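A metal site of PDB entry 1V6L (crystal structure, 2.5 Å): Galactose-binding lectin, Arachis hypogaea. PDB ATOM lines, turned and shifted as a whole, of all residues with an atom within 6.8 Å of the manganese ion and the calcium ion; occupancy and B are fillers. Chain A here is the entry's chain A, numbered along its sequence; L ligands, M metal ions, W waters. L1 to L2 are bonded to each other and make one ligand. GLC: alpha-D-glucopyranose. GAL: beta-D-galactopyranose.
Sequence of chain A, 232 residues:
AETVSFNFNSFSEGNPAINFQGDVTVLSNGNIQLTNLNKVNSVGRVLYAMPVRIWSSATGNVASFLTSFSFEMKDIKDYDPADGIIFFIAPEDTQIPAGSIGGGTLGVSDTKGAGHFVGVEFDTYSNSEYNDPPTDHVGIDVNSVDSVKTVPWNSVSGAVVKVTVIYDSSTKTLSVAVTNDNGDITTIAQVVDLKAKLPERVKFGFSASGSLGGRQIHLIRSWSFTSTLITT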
ATOM      1  N   ASP A  83     -29.389 -21.710  -9.624  1.00  0.00           N
ATOM      2  CA  ASP A  83     -28.796 -22.729  -8.741  1.00  0.00           C
ATOM      3  C   ASP A  83     -29.981 -23.542  -8.195  1.00  0.00           C
ATOM      4  O   ASP A  83     -29.988 -24.777  -8.214  1.00  0.00           O
ATOM      5  CB  ASP A  83     -27.987 -22.043  -7.626  1.00  0.00           C
ATOM      6  CG  ASP A  83     -26.552 -21.767  -8.046  1.00  0.00           C
ATOM      7  OD1 ASP A  83     -25.748 -22.719  -8.055  1.00  0.00           O
ATOM      8  OD2 ASP A  83     -26.215 -20.607  -8.368  1.00  0.00           O
ATOM      9  N   GLY A 103     -24.849 -18.659  -5.446  1.00  0.00           N
ATOM     10  CA  GLY A 103     -24.513 -19.951  -6.039  1.00  0.00           C
ATOM     11  C   GLY A 103     -24.991 -21.125  -5.205  1.00  0.00           C
ATOM     12  O   GLY A 103     -26.131 -21.150  -4.741  1.00  0.00           O
ATOM     13  N   GLY A 104     -24.102 -22.102  -5.008  1.00  0.00           N
ATOM     14  CA  GLY A 104     -24.429 -23.285  -4.242  1.00  0.00           C
ATOM     15  C   GLY A 104     -24.894 -23.084  -2.817  1.00  0.00           C
ATOM     16  O   GLY A 104     -25.552 -23.961  -2.253  1.00  0.00           O
ATOM     17  N   THR A 105     -24.576 -21.937  -2.211  1.00  0.00           N
ATOM     18  CA  THR A 105     -24.984 -21.687  -0.828  1.00  0.00           C
ATOM     19  C   THR A 105     -26.492 -21.523  -0.721  1.00  0.00           C
ATOM     20  O   THR A 105     -27.051 -21.613   0.375  1.00  0.00           O
ATOM     21  CB  THR A 105     -24.313 -20.421  -0.256  1.00  0.00           C
ATOM     22  OG1 THR A 105     -24.854 -19.251  -0.890  1.00  0.00           O
ATOM     23  CG2 THR A 105     -22.824 -20.467  -0.487  1.00  0.00           C
ATOM     24  N   LEU A 106     -27.146 -21.278  -1.855  1.00  0.00           N
ATOM     25  CA  LEU A 106     -28.597 -21.109  -1.893  1.00  0.00           C
ATOM     26  C   LEU A 106     -29.097 -19.933  -1.053  1.00  0.00           C
ATOM     27  O   LEU A 106     -30.283 -19.826  -0.765  1.00  0.00           O
ATOM     28  CB  LEU A 106     -29.305 -22.394  -1.446  1.00  0.00           C
ATOM     29  CG  LEU A 106     -29.007 -23.635  -2.305  1.00  0.00           C
ATOM     30  CD1 LEU A 106     -29.781 -24.830  -1.758  1.00  0.00           C
ATOM     31  CD2 LEU A 106     -29.409 -23.371  -3.744  1.00  0.00           C
ATOM     32  N   GLU A 121     -34.420 -28.423  -0.077  1.00  0.00           N
ATOM     33  CA  GLU A 121     -33.870 -27.806  -1.278  1.00  0.00           C
ATOM     34  C   GLU A 121     -34.208 -28.479  -2.596  1.00  0.00           C
ATOM     35  O   GLU A 121     -34.345 -29.695  -2.697  1.00  0.00           O
ATOM     36  CB  GLU A 121     -32.354 -27.716  -1.163  1.00  0.00           C
ATOM     37  CG  GLU A 121     -31.669 -29.067  -1.114  1.00  0.00           C
ATOM     38  CD  GLU A 121     -30.177 -28.957  -1.258  1.00  0.00           C
ATOM     39  OE1 GLU A 121     -29.546 -28.230  -0.467  1.00  0.00           O
ATOM     40  OE2 GLU A 121     -29.628 -29.599  -2.171  1.00  0.00           O
ATOM     41  N   PHE A 122     -34.318 -27.634  -3.617  1.00  0.00           N
ATOM     42  CA  PHE A 122     -34.605 -28.048  -4.974  1.00  0.00           C
ATOM     43  C   PHE A 122     -33.406 -27.493  -5.708  1.00  0.00           C
ATOM     44  O   PHE A 122     -33.422 -26.404  -6.275  1.00  0.00           O
ATOM     45  CB  PHE A 122     -35.923 -27.416  -5.386  1.00  0.00           C
ATOM     46  CG  PHE A 122     -37.061 -27.778  -4.464  1.00  0.00           C
ATOM     47  CD1 PHE A 122     -37.865 -28.878  -4.732  1.00  0.00           C
ATOM     48  CD2 PHE A 122     -37.256 -27.064  -3.274  1.00  0.00           C
ATOM     49  CE1 PHE A 122     -38.854 -29.269  -3.821  1.00  0.00           C
ATOM     50  CE2 PHE A 122     -38.238 -27.460  -2.363  1.00  0.00           C
ATOM     51  CZ  PHE A 122     -39.034 -28.567  -2.631  1.00  0.00           C
ATOM     52  N   ASP A 123     -32.335 -28.289  -5.646  1.00  0.00           N
ATOM     53  CA  ASP A 123     -31.033 -27.967  -6.215  1.00  0.00           C
ATOM     54  C   ASP A 123     -30.897 -28.335  -7.683  1.00  0.00           C
ATOM     55  O   ASP A 123     -31.078 -29.493  -8.060  1.00  0.00           O
ATOM     56  CB  ASP A 123     -29.986 -28.704  -5.407  1.00  0.00           C
ATOM     57  CG  ASP A 123     -28.679 -28.013  -5.428  1.00  0.00           C
ATOM     58  OD1 ASP A 123     -28.321 -27.436  -6.485  1.00  0.00           O
ATOM     59  OD2 ASP A 123     -27.988 -28.046  -4.396  1.00  0.00           O
ATOM     60  N   THR A 124     -30.532 -27.352  -8.516  1.00  0.00           N
ATOM     61  CA  THR A 124     -30.404 -27.576  -9.944  1.00  0.00           C
ATOM     62  C   THR A 124     -28.986 -27.566 -10.497  1.00  0.00           C
ATOM     63  O   THR A 124     -28.783 -27.703 -11.706  1.00  0.00           O
ATOM     64  CB  THR A 124     -31.217 -26.538 -10.738  1.00  0.00           C
ATOM     65  OG1 THR A 124     -30.671 -25.231 -10.502  1.00  0.00           O
ATOM     66  CG2 THR A 124     -32.676 -26.580 -10.303  1.00  0.00           C
ATOM     67  N   TYR A 125     -28.000 -27.408  -9.631  1.00  0.00           N
ATOM     68  CA  TYR A 125     -26.621 -27.427 -10.052  1.00  0.00           C
ATOM     69  C   TYR A 125     -25.826 -28.305  -9.091  1.00  0.00           C
ATOM     70  O   TYR A 125     -26.132 -28.347  -7.898  1.00  0.00           O
ATOM     71  CB  TYR A 125     -26.020 -26.024 -10.087  1.00  0.00           C
ATOM     72  CG  TYR A 125     -24.595 -26.020 -10.567  1.00  0.00           C
ATOM     73  CD1 TYR A 125     -23.535 -26.221  -9.682  1.00  0.00           C
ATOM     74  CD2 TYR A 125     -24.297 -25.893 -11.930  1.00  0.00           C
ATOM     75  CE1 TYR A 125     -22.217 -26.297 -10.137  1.00  0.00           C
ATOM     76  CE2 TYR A 125     -22.992 -25.968 -12.397  1.00  0.00           C
ATOM     77  CZ  TYR A 125     -21.957 -26.167 -11.496  1.00  0.00           C
ATOM     78  OH  TYR A 125     -20.655 -26.246 -11.944  1.00  0.00           O
ATOM     79  N   SER A 126     -24.826 -29.009  -9.594  1.00  0.00           N
ATOM     80  CA  SER A 126     -24.054 -29.896  -8.743  1.00  0.00           C
ATOM     81  C   SER A 126     -22.748 -29.303  -8.203  1.00  0.00           C
ATOM     82  O   SER A 126     -21.716 -29.310  -8.881  1.00  0.00           O
ATOM     83  CB  SER A 126     -23.775 -31.191  -9.524  1.00  0.00           C
ATOM     84  OG  SER A 126     -23.210 -32.181  -8.691  1.00  0.00           O
ATOM     85  N   ASN A 127     -22.795 -28.784  -6.977  1.00  0.00           N
ATOM     86  CA  ASN A 127     -21.606 -28.206  -6.347  1.00  0.00           C
ATOM     87  C   ASN A 127     -20.838 -29.280  -5.611  1.00  0.00           C
ATOM     88  O   ASN A 127     -21.238 -29.707  -4.529  1.00  0.00           O
ATOM     89  CB  ASN A 127     -21.987 -27.122  -5.350  1.00  0.00           C
ATOM     90  CG  ASN A 127     -22.518 -25.880  -6.018  1.00  0.00           C
ATOM     91  OD1 ASN A 127     -23.650 -25.858  -6.477  1.00  0.00           O
ATOM     92  ND2 ASN A 127     -21.698 -24.835  -6.081  1.00  0.00           N
ATOM     93  N   SER A 128     -19.721 -29.710  -6.199  1.00  0.00           N
ATOM     94  CA  SER A 128     -18.900 -30.738  -5.598  1.00  0.00           C
ATOM     95  C   SER A 128     -18.377 -30.325  -4.231  1.00  0.00           C
ATOM     96  O   SER A 128     -18.175 -31.155  -3.356  1.00  0.00           O
ATOM     97  CB  SER A 128     -17.738 -31.098  -6.517  1.00  0.00           C
ATOM     98  OG  SER A 128     -16.995 -29.942  -6.849  1.00  0.00           O
ATOM     99  N   TYR A 130     -19.880 -29.099  -1.971  1.00  0.00           N
ATOM    100  CA  TYR A 130     -20.882 -29.397  -0.948  1.00  0.00           C
ATOM    101  C   TYR A 130     -21.409 -30.820  -1.102  1.00  0.00           C
ATOM    102  O   TYR A 130     -22.458 -31.170  -0.566  1.00  0.00           O
ATOM    103  CB  TYR A 130     -22.045 -28.402  -1.036  1.00  0.00           C
ATOM    104  CG  TYR A 130     -21.618 -26.957  -0.968  1.00  0.00           C
ATOM    105  CD1 TYR A 130     -20.811 -26.487   0.068  1.00  0.00           C
ATOM    106  CD2 TYR A 130     -22.003 -26.048  -1.963  1.00  0.00           C
ATOM    107  CE1 TYR A 130     -20.405 -25.142   0.121  1.00  0.00           C
ATOM    108  CE2 TYR A 130     -21.610 -24.717  -1.915  1.00  0.00           C
ATOM    109  CZ  TYR A 130     -20.802 -24.278  -0.875  1.00  0.00           C
ATOM    110  OH  TYR A 130     -20.381 -22.961  -0.857  1.00  0.00           O
ATOM    111  N   ASN A 131     -20.660 -31.632  -1.839  1.00  0.00           N
ATOM    112  CA  ASN A 131     -21.002 -33.039  -2.059  1.00  0.00           C
ATOM    113  C   ASN A 131     -22.368 -33.302  -2.684  1.00  0.00           C
ATOM    114  O   ASN A 131     -23.048 -34.264  -2.319  1.00  0.00           O
ATOM    115  CB  ASN A 131     -20.885 -33.817  -0.753  1.00  0.00           C
ATOM    116  CG  ASN A 131     -19.491 -33.735  -0.152  1.00  0.00           C
ATOM    117  OD1 ASN A 131     -18.496 -34.015  -0.823  1.00  0.00           O
ATOM    118  ND2 ASN A 131     -19.409 -33.358   1.119  1.00  0.00           N
ATOM    119  N   ASP A 132     -22.782 -32.457  -3.625  1.00  0.00           N
ATOM    120  CA  ASP A 132     -24.065 -32.640  -4.290  1.00  0.00           C
ATOM    121  C   ASP A 132     -24.087 -33.901  -5.128  1.00  0.00           C
ATOM    122  O   ASP A 132     -23.060 -34.360  -5.614  1.00  0.00           O
ATOM    123  CB  ASP A 132     -24.376 -31.492  -5.251  1.00  0.00           C
ATOM    124  CG  ASP A 132     -24.906 -30.274  -4.563  1.00  0.00           C
ATOM    125  OD1 ASP A 132     -25.605 -30.419  -3.546  1.00  0.00           O
ATOM    126  OD2 ASP A 132     -24.645 -29.170  -5.077  1.00  0.00           O
ATOM    127  N   PRO A 133     -25.282 -34.491  -5.305  1.00  0.00           N
ATOM    128  CA  PRO A 133     -25.347 -35.694  -6.127  1.00  0.00           C
ATOM    129  C   PRO A 133     -24.991 -35.178  -7.531  1.00  0.00           C
ATOM    130  O   PRO A 133     -24.852 -33.973  -7.733  1.00  0.00           O
ATOM    131  CB  PRO A 133     -26.814 -36.096  -6.032  1.00  0.00           C
ATOM    132  CG  PRO A 133     -27.192 -35.626  -4.647  1.00  0.00           C
ATOM    133  CD  PRO A 133     -26.535 -34.281  -4.549  1.00  0.00           C
ATOM    134  N   HIS A 137     -31.699 -32.453  -7.773  1.00  0.00           N
ATOM    135  CA  HIS A 137     -32.180 -33.235  -6.658  1.00  0.00           C
ATOM    136  C   HIS A 137     -32.930 -32.444  -5.603  1.00  0.00           C
ATOM    137  O   HIS A 137     -32.927 -31.214  -5.596  1.00  0.00           O
ATOM    138  CB  HIS A 137     -30.988 -33.910  -5.987  1.00  0.00           C
ATOM    139  CG  HIS A 137     -29.946 -32.932  -5.536  1.00  0.00           C
ATOM    140  ND1 HIS A 137     -29.089 -32.313  -6.422  1.00  0.00           N
ATOM    141  CD2 HIS A 137     -29.652 -32.448  -4.308  1.00  0.00           C
ATOM    142  CE1 HIS A 137     -28.310 -31.476  -5.757  1.00  0.00           C
ATOM    143  NE2 HIS A 137     -28.626 -31.545  -4.468  1.00  0.00           N
ATOM    144  N   VAL A 138     -33.564 -33.187  -4.715  1.00  0.00           N
ATOM    145  CA  VAL A 138     -34.279 -32.615  -3.598  1.00  0.00           C
ATOM    146  C   VAL A 138     -33.480 -33.107  -2.397  1.00  0.00           C
ATOM    147  O   VAL A 138     -33.056 -34.270  -2.354  1.00  0.00           O
ATOM    148  CB  VAL A 138     -35.707 -33.140  -3.521  1.00  0.00           C
ATOM    149  CG1 VAL A 138     -36.398 -32.589  -2.290  1.00  0.00           C
ATOM    150  CG2 VAL A 138     -36.467 -32.757  -4.780  1.00  0.00           C
ATOM    151  N   GLY A 139     -33.238 -32.235  -1.427  1.00  0.00           N
ATOM    152  CA  GLY A 139     -32.469 -32.669  -0.271  1.00  0.00           C
ATOM    153  C   GLY A 139     -32.916 -32.017   1.005  1.00  0.00           C
ATOM    154  O   GLY A 139     -33.451 -30.906   0.994  1.00  0.00           O
ATOM    155  N   ASP A 141     -31.823 -30.359   4.345  1.00  0.00           N
ATOM    156  CA  ASP A 141     -30.643 -29.728   4.891  1.00  0.00           C
ATOM    157  C   ASP A 141     -30.798 -29.399   6.358  1.00  0.00           C
ATOM    158  O   ASP A 141     -31.852 -28.924   6.790  1.00  0.00           O
ATOM    159  CB  ASP A 141     -30.300 -28.451   4.128  1.00  0.00           C
ATOM    160  CG  ASP A 141     -29.998 -28.702   2.663  1.00  0.00           C
ATOM    161  OD1 ASP A 141     -29.534 -29.816   2.329  1.00  0.00           O
ATOM    162  OD2 ASP A 141     -30.216 -27.784   1.846  1.00  0.00           O
ATOM    163  N   VAL A 145     -25.665 -27.047   3.468  1.00  0.00           N
ATOM    164  CA  VAL A 145     -26.200 -27.306   2.121  1.00  0.00           C
ATOM    165  C   VAL A 145     -25.653 -28.644   1.681  1.00  0.00           C
ATOM    166  O   VAL A 145     -25.880 -29.099   0.555  1.00  0.00           O
ATOM    167  CB  VAL A 145     -25.794 -26.214   1.122  1.00  0.00           C
ATOM    168  CG1 VAL A 145     -26.556 -24.955   1.424  1.00  0.00           C
ATOM    169  CG2 VAL A 145     -24.292 -25.986   1.192  1.00  0.00           C
ATOM    170  N   ASP A 146     -24.881 -29.256   2.570  1.00  0.00           N
ATOM    171  CA  ASP A 146     -24.344 -30.577   2.329  1.00  0.00           C
ATOM    172  C   ASP A 146     -25.444 -31.416   2.968  1.00  0.00           C
ATOM    173  O   ASP A 146     -25.392 -31.762   4.148  1.00  0.00           O
ATOM    174  CB  ASP A 146     -23.040 -30.784   3.069  1.00  0.00           C
ATOM    175  CG  ASP A 146     -22.408 -32.117   2.749  1.00  0.00           C
ATOM    176  OD1 ASP A 146     -23.135 -33.035   2.295  1.00  0.00           O
ATOM    177  OD2 ASP A 146     -21.187 -32.264   2.968  1.00  0.00           O
ATOM    178  N   SER A 147     -26.466 -31.693   2.173  1.00  0.00           N
ATOM    179  CA  SER A 147     -27.637 -32.442   2.590  1.00  0.00           C
ATOM    180  C   SER A 147     -27.414 -33.707   3.405  1.00  0.00           C
ATOM    181  O   SER A 147     -26.512 -34.496   3.137  1.00  0.00           O
ATOM    182  CB  SER A 147     -28.481 -32.770   1.370  1.00  0.00           C
ATOM    183  OG  SER A 147     -28.791 -31.592   0.655  1.00  0.00           O
ATOM    184  N   THR A 150     -30.481 -36.831   0.141  1.00  0.00           N
ATOM    185  CA  THR A 150     -30.959 -36.303  -1.129  1.00  0.00           C
ATOM    186  C   THR A 150     -31.664 -37.408  -1.910  1.00  0.00           C
ATOM    187  O   THR A 150     -31.515 -38.586  -1.598  1.00  0.00           O
ATOM    188  CB  THR A 150     -29.809 -35.774  -2.012  1.00  0.00           C
ATOM    189  OG1 THR A 150     -28.897 -36.843  -2.288  1.00  0.00           O
ATOM    190  CG2 THR A 150     -29.080 -34.625  -1.331  1.00  0.00           C
HETATM  191  C1  GLC L   1     -16.782 -18.982 -12.718  1.00  0.00           C
HETATM  192  C2  GLC L   1     -18.244 -18.838 -13.179  1.00  0.00           C
HETATM  193  C3  GLC L   1     -19.202 -19.055 -11.996  1.00  0.00           C
HETATM  194  C4  GLC L   1     -18.887 -20.381 -11.301  1.00  0.00           C
HETATM  195  C5  GLC L   1     -17.420 -20.411 -10.899  1.00  0.00           C
HETATM  196  C6  GLC L   1     -17.013 -21.722 -10.237  1.00  0.00           C
HETATM  197  O1  GLC L   1     -16.485 -17.985 -11.805  1.00  0.00           O
HETATM  198  O2  GLC L   1     -18.446 -17.551 -13.736  1.00  0.00           O
HETATM  199  O3  GLC L   1     -20.541 -19.059 -12.456  1.00  0.00           O
HETATM  200  O4  GLC L   1     -19.729 -20.524 -10.144  1.00  0.00           O
HETATM  201  O5  GLC L   1     -16.585 -20.246 -12.063  1.00  0.00           O
HETATM  202  O6  GLC L   1     -17.399 -22.823 -11.032  1.00  0.00           O
HETATM  203  C1  GAL L   2     -20.559 -21.642 -10.119  1.00  0.00           C
HETATM  204  C2  GAL L   2     -21.317 -21.674  -8.788  1.00  0.00           C
HETATM  205  C3  GAL L   2     -22.321 -22.840  -8.784  1.00  0.00           C
HETATM  206  C4  GAL L   2     -23.231 -22.739 -10.007  1.00  0.00           C
HETATM  207  C5  GAL L   2     -22.391 -22.673 -11.285  1.00  0.00           C
HETATM  208  C6  GAL L   2     -23.249 -22.480 -12.509  1.00  0.00           C
HETATM  209  O2  GAL L   2     -20.413 -21.828  -7.703  1.00  0.00           O
HETATM  210  O3  GAL L   2     -23.091 -22.809  -7.597  1.00  0.00           O
HETATM  211  O4  GAL L   2     -24.029 -21.566  -9.906  1.00  0.00           O
HETATM  212  O5  GAL L   2     -21.477 -21.551 -11.221  1.00  0.00           O
HETATM  213  O6  GAL L   2     -22.503 -22.678 -13.706  1.00  0.00           O
HETATM  214 MN    MN M   1     -27.691 -29.902  -3.124  1.00  0.00          MN
HETATM  215 CA    CA M   2     -25.832 -27.004  -5.673  1.00  0.00          CA
HETATM  216  O   HOH W   1     -25.728 -26.366  -3.127  1.00  0.00           O
HETATM  217  O   HOH W   2     -27.543 -31.596  -1.677  1.00  0.00           O
HETATM  218  O   HOH W   3     -26.997 -28.250  -1.499  1.00  0.00           O
HETATM  219  O   HOH W   4     -26.902 -24.700  -6.469  1.00  0.00           O
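The manganese ion is bound by the side-chain carboxylate of Glu 121 (2.2 Å), the side-chain carboxylate of Asp 132 (2.2 Å), water W2 (2.2 Å), the side-chain carboxylate of Asp 123 (2.3 Å), a ring nitrogen (NE2) of His 137 (2.3 Å) and water W3 (2.4 Å). The manganese ion has six donor atoms within binding distance.
O3 of GAL L2 is in hydrogen-bond range of ND2 of Asn 127, at 2.9 Å. N of Gly 104 lies within hydrogen-bond range of O3 of GAL L2 (2.9 Å). The side-chain carboxylate (OD1) of Asp 83 lies within hydrogen-bond range of an oxygen (O3) of GAL L2 (2.7 Å).
The side-chain carboxylate (OE1) of Glu 121 lies close to the side-chain carboxylate (OD2) of Asp 141 (2.4 Å). The backbone carbonyl oxygen of Gly 139 is in hydrogen-bond range of the backbone NH of Glu 121, 2.9 Å away.
Within 4 Å of the manganese ion: Glu 121, Asp 123, Asp 132 and His 137.
OD2 of Asp 132 binds the calcium ion (2.5 Å). OD1 of Asn 127 binds the calcium ion. The calcium ion is bound by O of Tyr 125, at 2.6 Å. Water W1 is bound to the calcium ion (2.6 Å). The calcium ion is bound by the side-chain carboxylate (OD1) of Asp 123 (2.7 Å). The calcium ion is bound by water W4. The side-chain carboxylate (OD2) of Asp 123 binds the calcium ion (2.7 Å). The calcium ion has seven donor atoms within binding distance.
Of the 25 residues printed, 4 come within 4 Å of the calcium ion.
Water W3 lies within hydrogen-bond range of the backbone carbonyl oxygen of Val 145 (2.5 Å) and the side-chain carboxylate of Glu 121 (2.8 Å).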
